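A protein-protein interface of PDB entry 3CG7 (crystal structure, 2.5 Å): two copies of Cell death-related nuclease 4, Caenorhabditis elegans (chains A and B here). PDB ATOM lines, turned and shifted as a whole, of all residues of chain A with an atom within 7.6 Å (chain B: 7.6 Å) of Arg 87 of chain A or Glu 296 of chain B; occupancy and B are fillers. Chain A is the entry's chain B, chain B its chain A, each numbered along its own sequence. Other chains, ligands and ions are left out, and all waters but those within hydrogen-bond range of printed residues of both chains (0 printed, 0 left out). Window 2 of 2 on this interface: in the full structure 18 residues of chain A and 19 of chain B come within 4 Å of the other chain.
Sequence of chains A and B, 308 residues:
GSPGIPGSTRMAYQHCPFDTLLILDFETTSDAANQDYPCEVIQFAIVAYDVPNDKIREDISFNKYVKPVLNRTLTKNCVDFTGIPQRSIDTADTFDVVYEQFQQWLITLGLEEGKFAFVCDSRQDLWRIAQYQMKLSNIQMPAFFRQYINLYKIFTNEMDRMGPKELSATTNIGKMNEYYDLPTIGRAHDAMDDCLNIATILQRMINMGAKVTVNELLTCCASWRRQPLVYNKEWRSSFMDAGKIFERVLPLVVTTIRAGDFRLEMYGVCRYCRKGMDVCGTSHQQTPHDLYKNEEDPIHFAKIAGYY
The side-chain carboxylate (OE2) of Glu 296 of chain B lies within salt-bridge range of the guanidinium group (NH1) of Arg 87 of chain A (3.8 Å).
OD1 of Asp 90 of chain A lies within hydrogen-bond range of ND1 of His 300 of chain B, 2.7 Å away.
The guanidinium group (NH2) of Arg 236 of chain B lies within hydrogen-bond range of the backbone carbonyl oxygen (O) of Pro 298 of chain B (2.8 Å).
OD1 of Asn 294 of chain B lies close to N of Glu 296 of chain B.
N of Leu 74 of chain A sits at hydrogen-bond distance from OE1 of Gln 86 of chain A (2.8 Å).
NE2 of Gln 86 of chain A sits at hydrogen-bond distance from OD2 of Asp 90 of chain A (2.9 Å).
O of Arg 87 of chain A is in hydrogen-bond range of OG1 of Thr 91 of chain A (3.3 Å).
Among the printed residues, merely in contact across the chains: Gln 86 of chain A with His 300 of chain B (3.4 Å), Arg 87 of chain A with Glu 295 of chain B (3.8 Å), Arg 87 of chain A with Pro 298 of chain B (3.8 Å), Asp 90 of chain A with Lys 303 of chain B (3.7 Å) and Thr 91 of chain A with Lys 303 of chain B (3.5 Å).
Tyr 65 of chain A touches none of the printed residues of chain B.
Printed residues of chain B within 4 Å of Gln 86 of chain A: His 300 (3.4 Å).
Arg 87 of chain A touches three residues of chain B.
Of the printed residues of chain B, Asp 90 of chain A touches His 300 and Lys 303.
Glu 296 of chain B touches just one residue of chain A: Arg 87 (3.6 Å).
Of the printed residues of chain A, Pro 298 of chain B touches Arg 87 (3.8 Å).
Of the printed residues of chain A, Lys 303 of chain B touches Asp 90 and Thr 91.
The nearest residue of chain A that does not touch Glu 296 of chain B is Pro 85 of chain A (7.0 Å).
The nearest printed residue of chain B that does not touch Thr 91 of chain A is Glu 295 of chain B (6.6 Å).
Hydrophobic or aromatic side chains of chain B within 4 Å of the printed part of chain A: Pro 298 and His 300.
Of the 11 printed residues of chain A, 4 touch a printed residue of chain B.
Printed residues of chain A that touch a printed residue of chain B: Gln 86, Arg 87, Asp 90 and Thr 91.
Among the printed residues, 7 pairs touch across the chains.
No position is printed for both chains.
Of the 7 pairs that touch across the chains among the printed residues, none has its exchanged pair printed and touching as well.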
ATOM      1  N   TYR A  65     -33.206 -25.755  22.971  1.00  0.00           N
ATOM      2  CA  TYR A  65     -32.595 -25.663  21.655  1.00  0.00           C
ATOM      3  C   TYR A  65     -31.676 -26.854  21.459  1.00  0.00           C
ATOM      4  O   TYR A  65     -31.255 -27.493  22.433  1.00  0.00           O
ATOM      5  CB  TYR A  65     -31.808 -24.362  21.511  1.00  0.00           C
ATOM      6  CG  TYR A  65     -32.689 -23.151  21.382  1.00  0.00           C
ATOM      7  CD1 TYR A  65     -33.568 -23.027  20.298  1.00  0.00           C
ATOM      8  CD2 TYR A  65     -32.647 -22.123  22.331  1.00  0.00           C
ATOM      9  CE1 TYR A  65     -34.387 -21.923  20.166  1.00  0.00           C
ATOM     10  CE2 TYR A  65     -33.465 -21.005  22.206  1.00  0.00           C
ATOM     11  CZ  TYR A  65     -34.331 -20.916  21.124  1.00  0.00           C
ATOM     12  OH  TYR A  65     -35.150 -19.828  20.975  1.00  0.00           O
ATOM     13  N   LEU A  74     -27.421 -22.464  10.179  1.00  0.00           N
ATOM     14  CA  LEU A  74     -28.811 -22.347   9.791  1.00  0.00           C
ATOM     15  C   LEU A  74     -28.935 -21.546   8.521  1.00  0.00           C
ATOM     16  O   LEU A  74     -28.394 -20.456   8.386  1.00  0.00           O
ATOM     17  CB  LEU A  74     -29.636 -21.696  10.905  1.00  0.00           C
ATOM     18  CG  LEU A  74     -30.520 -22.544  11.830  1.00  0.00           C
ATOM     19  CD1 LEU A  74     -30.013 -23.972  12.025  1.00  0.00           C
ATOM     20  CD2 LEU A  74     -30.721 -21.838  13.177  1.00  0.00           C
ATOM     21  N   ILE A  84     -35.774 -18.844  14.828  1.00  0.00           N
ATOM     22  CA  ILE A  84     -34.644 -19.200  15.685  1.00  0.00           C
ATOM     23  C   ILE A  84     -33.347 -18.582  15.145  1.00  0.00           C
ATOM     24  O   ILE A  84     -32.993 -18.798  13.981  1.00  0.00           O
ATOM     25  CB  ILE A  84     -34.493 -20.730  15.816  1.00  0.00           C
ATOM     26  CG1 ILE A  84     -35.781 -21.340  16.380  1.00  0.00           C
ATOM     27  CG2 ILE A  84     -33.281 -21.086  16.681  1.00  0.00           C
ATOM     28  CD1 ILE A  84     -36.024 -22.788  15.988  1.00  0.00           C
ATOM     29  N   PRO A  85     -32.649 -17.784  15.981  1.00  0.00           N
ATOM     30  CA  PRO A  85     -31.377 -17.187  15.552  1.00  0.00           C
ATOM     31  C   PRO A  85     -30.195 -18.125  15.770  1.00  0.00           C
ATOM     32  O   PRO A  85     -30.242 -18.993  16.659  1.00  0.00           O
ATOM     33  CB  PRO A  85     -31.255 -15.959  16.455  1.00  0.00           C
ATOM     34  CG  PRO A  85     -31.944 -16.373  17.730  1.00  0.00           C
ATOM     35  CD  PRO A  85     -33.019 -17.373  17.355  1.00  0.00           C
ATOM     36  N   GLN A  86     -29.143 -17.934  14.972  1.00  0.00           N
ATOM     37  CA  GLN A  86     -27.939 -18.776  15.013  1.00  0.00           C
ATOM     38  C   GLN A  86     -27.310 -18.923  16.400  1.00  0.00           C
ATOM     39  O   GLN A  86     -26.907 -20.023  16.781  1.00  0.00           O
ATOM     40  CB  GLN A  86     -26.890 -18.283  14.004  1.00  0.00           C
ATOM     41  CG  GLN A  86     -25.684 -19.212  13.851  1.00  0.00           C
ATOM     42  CD  GLN A  86     -26.046 -20.522  13.163  1.00  0.00           C
ATOM     43  OE1 GLN A  86     -26.681 -20.522  12.107  1.00  0.00           O
ATOM     44  NE2 GLN A  86     -25.638 -21.645  13.759  1.00  0.00           N
ATOM     45  N   ARG A  87     -27.222 -17.823  17.144  1.00  0.00           N
ATOM     46  CA  ARG A  87     -26.638 -17.836  18.496  1.00  0.00           C
ATOM     47  C   ARG A  87     -27.250 -18.891  19.419  1.00  0.00           C
ATOM     48  O   ARG A  87     -26.520 -19.560  20.163  1.00  0.00           O
ATOM     49  CB  ARG A  87     -26.712 -16.450  19.151  1.00  0.00           C
ATOM     50  CG  ARG A  87     -28.132 -15.943  19.444  1.00  0.00           C
ATOM     51  CD  ARG A  87     -28.126 -14.497  19.928  1.00  0.00           C
ATOM     52  NE  ARG A  87     -29.473 -13.932  19.951  1.00  0.00           N
ATOM     53  CZ  ARG A  87     -30.292 -13.992  20.998  1.00  0.00           C
ATOM     54  NH1 ARG A  87     -29.910 -14.594  22.123  1.00  0.00           N
ATOM     55  NH2 ARG A  87     -31.502 -13.451  20.922  1.00  0.00           N
ATOM     56  N   SER A  88     -28.573 -19.054  19.353  1.00  0.00           N
ATOM     57  CA  SER A  88     -29.291 -19.990  20.225  1.00  0.00           C
ATOM     58  C   SER A  88     -28.940 -21.471  20.001  1.00  0.00           C
ATOM     59  O   SER A  88     -29.059 -22.278  20.927  1.00  0.00           O
ATOM     60  CB  SER A  88     -30.804 -19.783  20.116  1.00  0.00           C
ATOM     61  OG  SER A  88     -31.180 -18.521  20.633  1.00  0.00           O
ATOM     62  N   ILE A  89     -28.517 -21.827  18.786  1.00  0.00           N
ATOM     63  CA  ILE A  89     -28.078 -23.204  18.534  1.00  0.00           C
ATOM     64  C   ILE A  89     -26.562 -23.421  18.689  1.00  0.00           C
ATOM     65  O   ILE A  89     -26.121 -24.543  18.934  1.00  0.00           O
ATOM     66  CB  ILE A  89     -28.600 -23.797  17.184  1.00  0.00           C
ATOM     67  CG1 ILE A  89     -27.959 -23.109  15.991  1.00  0.00           C
ATOM     68  CG2 ILE A  89     -30.147 -23.749  17.092  1.00  0.00           C
ATOM     69  CD1 ILE A  89     -27.864 -24.011  14.810  1.00  0.00           C
ATOM     70  N   ASP A  90     -25.771 -22.357  18.559  1.00  0.00           N
ATOM     71  CA  ASP A  90     -24.325 -22.450  18.804  1.00  0.00           C
ATOM     72  C   ASP A  90     -24.003 -22.719  20.281  1.00  0.00           C
ATOM     73  O   ASP A  90     -22.982 -23.340  20.593  1.00  0.00           O
ATOM     74  CB  ASP A  90     -23.592 -21.189  18.318  1.00  0.00           C
ATOM     75  CG  ASP A  90     -23.514 -21.090  16.794  1.00  0.00           C
ATOM     76  OD1 ASP A  90     -23.063 -20.038  16.302  1.00  0.00           O
ATOM     77  OD2 ASP A  90     -23.896 -22.045  16.076  1.00  0.00           O
ATOM     78  N   THR A  91     -24.882 -22.259  21.178  1.00  0.00           N
ATOM     79  CA  THR A  91     -24.734 -22.502  22.624  1.00  0.00           C
ATOM     80  C   THR A  91     -25.498 -23.732  23.124  1.00  0.00           C
ATOM     81  O   THR A  91     -25.484 -24.032  24.318  1.00  0.00           O
ATOM     82  CB  THR A  91     -25.156 -21.268  23.483  1.00  0.00           C
ATOM     83  OG1 THR A  91     -26.502 -20.877  23.158  1.00  0.00           O
ATOM     84  CG2 THR A  91     -24.188 -20.085  23.274  1.00  0.00           C
ATOM     85  N   ALA A  92     -26.150 -24.445  22.208  1.00  0.00           N
ATOM     86  CA  ALA A  92     -27.008 -25.571  22.572  1.00  0.00           C
ATOM     87  C   ALA A  92     -26.239 -26.886  22.643  1.00  0.00           C
ATOM     88  O   ALA A  92     -25.131 -26.985  22.127  1.00  0.00           O
ATOM     89  CB  ALA A  92     -28.183 -25.686  21.592  1.00  0.00           C
ATOM     90  N   ARG B 236     -24.444  -8.770   7.703  1.00  0.00           N
ATOM     91  CA  ARG B 236     -24.624 -10.139   7.229  1.00  0.00           C
ATOM     92  C   ARG B 236     -25.277 -10.252   5.857  1.00  0.00           C
ATOM     93  O   ARG B 236     -25.244 -11.319   5.242  1.00  0.00           O
ATOM     94  CB  ARG B 236     -25.377 -10.971   8.274  1.00  0.00           C
ATOM     95  CG  ARG B 236     -24.574 -11.187   9.551  1.00  0.00           C
ATOM     96  CD  ARG B 236     -25.359 -11.931  10.605  1.00  0.00           C
ATOM     97  NE  ARG B 236     -24.559 -12.185  11.805  1.00  0.00           N
ATOM     98  CZ  ARG B 236     -24.404 -11.325  12.812  1.00  0.00           C
ATOM     99  NH1 ARG B 236     -24.986 -10.136  12.773  1.00  0.00           N
ATOM    100  NH2 ARG B 236     -23.655 -11.653  13.859  1.00  0.00           N
ATOM    101  N   LYS B 293     -17.660  -9.064  22.332  1.00  0.00           N
ATOM    102  CA  LYS B 293     -18.289  -8.679  23.608  1.00  0.00           C
ATOM    103  C   LYS B 293     -19.757  -9.089  23.736  1.00  0.00           C
ATOM    104  O   LYS B 293     -20.203  -9.477  24.819  1.00  0.00           O
ATOM    105  CB  LYS B 293     -18.160  -7.166  23.835  1.00  0.00           C
ATOM    106  CG  LYS B 293     -18.839  -6.286  22.758  1.00  0.00           C
ATOM    107  CD  LYS B 293     -18.995  -4.822  23.213  1.00  0.00           C
ATOM    108  CE  LYS B 293     -20.186  -4.636  24.164  1.00  0.00           C
ATOM    109  NZ  LYS B 293     -20.131  -3.328  24.885  1.00  0.00           N
ATOM    110  N   ASN B 294     -20.493  -9.011  22.628  1.00  0.00           N
ATOM    111  CA  ASN B 294     -21.954  -9.078  22.634  1.00  0.00           C
ATOM    112  C   ASN B 294     -22.534 -10.470  22.336  1.00  0.00           C
ATOM    113  O   ASN B 294     -22.734 -10.835  21.169  1.00  0.00           O
ATOM    114  CB  ASN B 294     -22.506  -8.033  21.647  1.00  0.00           C
ATOM    115  CG  ASN B 294     -24.008  -7.843  21.762  1.00  0.00           C
ATOM    116  OD1 ASN B 294     -24.655  -8.400  22.651  1.00  0.00           O
ATOM    117  ND2 ASN B 294     -24.572  -7.051  20.859  1.00  0.00           N
ATOM    118  N   GLU B 295     -22.825 -11.237  23.387  1.00  0.00           N
ATOM    119  CA  GLU B 295     -23.403 -12.584  23.215  1.00  0.00           C
ATOM    120  C   GLU B 295     -24.863 -12.565  22.717  1.00  0.00           C
ATOM    121  O   GLU B 295     -25.478 -13.622  22.521  1.00  0.00           O
ATOM    122  CB  GLU B 295     -23.232 -13.458  24.477  1.00  0.00           C
ATOM    123  CG  GLU B 295     -23.840 -12.896  25.765  1.00  0.00           C
ATOM    124  CD  GLU B 295     -22.845 -12.069  26.579  1.00  0.00           C
ATOM    125  OE1 GLU B 295     -22.820 -10.821  26.423  1.00  0.00           O
ATOM    126  OE2 GLU B 295     -22.086 -12.672  27.373  1.00  0.00           O
ATOM    127  N   GLU B 296     -25.401 -11.363  22.508  1.00  0.00           N
ATOM    128  CA  GLU B 296     -26.706 -11.180  21.866  1.00  0.00           C
ATOM    129  C   GLU B 296     -26.581 -10.945  20.355  1.00  0.00           C
ATOM    130  O   GLU B 296     -27.590 -10.899  19.645  1.00  0.00           O
ATOM    131  CB  GLU B 296     -27.493 -10.034  22.524  1.00  0.00           C
ATOM    132  CG  GLU B 296     -28.635 -10.481  23.458  1.00  0.00           C
ATOM    133  CD  GLU B 296     -28.151 -11.178  24.727  1.00  0.00           C
ATOM    134  OE1 GLU B 296     -27.517 -10.507  25.574  1.00  0.00           O
ATOM    135  OE2 GLU B 296     -28.421 -12.393  24.881  1.00  0.00           O
ATOM    136  N   ASP B 297     -25.346 -10.792  19.872  1.00  0.00           N
ATOM    137  CA  ASP B 297     -25.082 -10.656  18.432  1.00  0.00           C
ATOM    138  C   ASP B 297     -23.702 -11.211  18.023  1.00  0.00           C
ATOM    139  O   ASP B 297     -22.901 -10.489  17.428  1.00  0.00           O
ATOM    140  CB  ASP B 297     -25.239  -9.191  17.989  1.00  0.00           C
ATOM    141  CG  ASP B 297     -25.294  -9.033  16.473  1.00  0.00           C
ATOM    142  OD1 ASP B 297     -24.986  -7.927  15.974  1.00  0.00           O
ATOM    143  OD2 ASP B 297     -25.643 -10.007  15.770  1.00  0.00           O
ATOM    144  N   PRO B 298     -23.434 -12.504  18.314  1.00  0.00           N
ATOM    145  CA  PRO B 298     -22.092 -13.064  18.107  1.00  0.00           C
ATOM    146  C   PRO B 298     -21.774 -13.310  16.629  1.00  0.00           C
ATOM    147  O   PRO B 298     -22.690 -13.393  15.803  1.00  0.00           O
ATOM    148  CB  PRO B 298     -22.139 -14.406  18.862  1.00  0.00           C
ATOM    149  CG  PRO B 298     -23.462 -14.464  19.537  1.00  0.00           C
ATOM    150  CD  PRO B 298     -24.367 -13.534  18.801  1.00  0.00           C
ATOM    151  N   ILE B 299     -20.483 -13.401  16.307  1.00  0.00           N
ATOM    152  CA  ILE B 299     -20.042 -13.678  14.938  1.00  0.00           C
ATOM    153  C   ILE B 299     -19.986 -15.185  14.771  1.00  0.00           C
ATOM    154  O   ILE B 299     -19.076 -15.842  15.288  1.00  0.00           O
ATOM    155  CB  ILE B 299     -18.629 -13.086  14.628  1.00  0.00           C
ATOM    156  CG1 ILE B 299     -18.479 -11.622  15.098  1.00  0.00           C
ATOM    157  CG2 ILE B 299     -18.281 -13.266  13.150  1.00  0.00           C
ATOM    158  CD1 ILE B 299     -19.442 -10.624  14.490  1.00  0.00           C
ATOM    159  N   HIS B 300     -20.964 -15.733  14.057  1.00  0.00           N
ATOM    160  CA  HIS B 300     -21.073 -17.184  13.921  1.00  0.00           C
ATOM    161  C   HIS B 300     -19.813 -17.833  13.326  1.00  0.00           C
ATOM    162  O   HIS B 300     -19.297 -18.793  13.895  1.00  0.00           O
ATOM    163  CB  HIS B 300     -22.328 -17.579  13.135  1.00  0.00           C
ATOM    164  CG  HIS B 300     -22.365 -19.026  12.752  1.00  0.00           C
ATOM    165  ND1 HIS B 300     -22.278 -20.045  13.678  1.00  0.00           N
ATOM    166  CD2 HIS B 300     -22.479 -19.626  11.542  1.00  0.00           C
ATOM    167  CE1 HIS B 300     -22.333 -21.209  13.056  1.00  0.00           C
ATOM    168  NE2 HIS B 300     -22.461 -20.982  11.759  1.00  0.00           N
ATOM    169  N   LYS B 303     -17.023 -17.978  15.769  1.00  0.00           N
ATOM    170  CA  LYS B 303     -17.238 -18.942  16.845  1.00  0.00           C
ATOM    171  C   LYS B 303     -16.998 -20.412  16.463  1.00  0.00           C
ATOM    172  O   LYS B 303     -16.213 -21.068  17.140  1.00  0.00           O
ATOM    173  CB  LYS B 303     -18.583 -18.739  17.561  1.00  0.00           C
ATOM    174  CG  LYS B 303     -18.410 -18.739  19.084  1.00  0.00           C
ATOM    175  CD  LYS B 303     -19.731 -18.677  19.833  1.00  0.00           C
ATOM    176  CE  LYS B 303     -20.230 -20.081  20.197  1.00  0.00           C
ATOM    177  NZ  LYS B 303     -21.444 -19.999  21.042  1.00  0.00           N
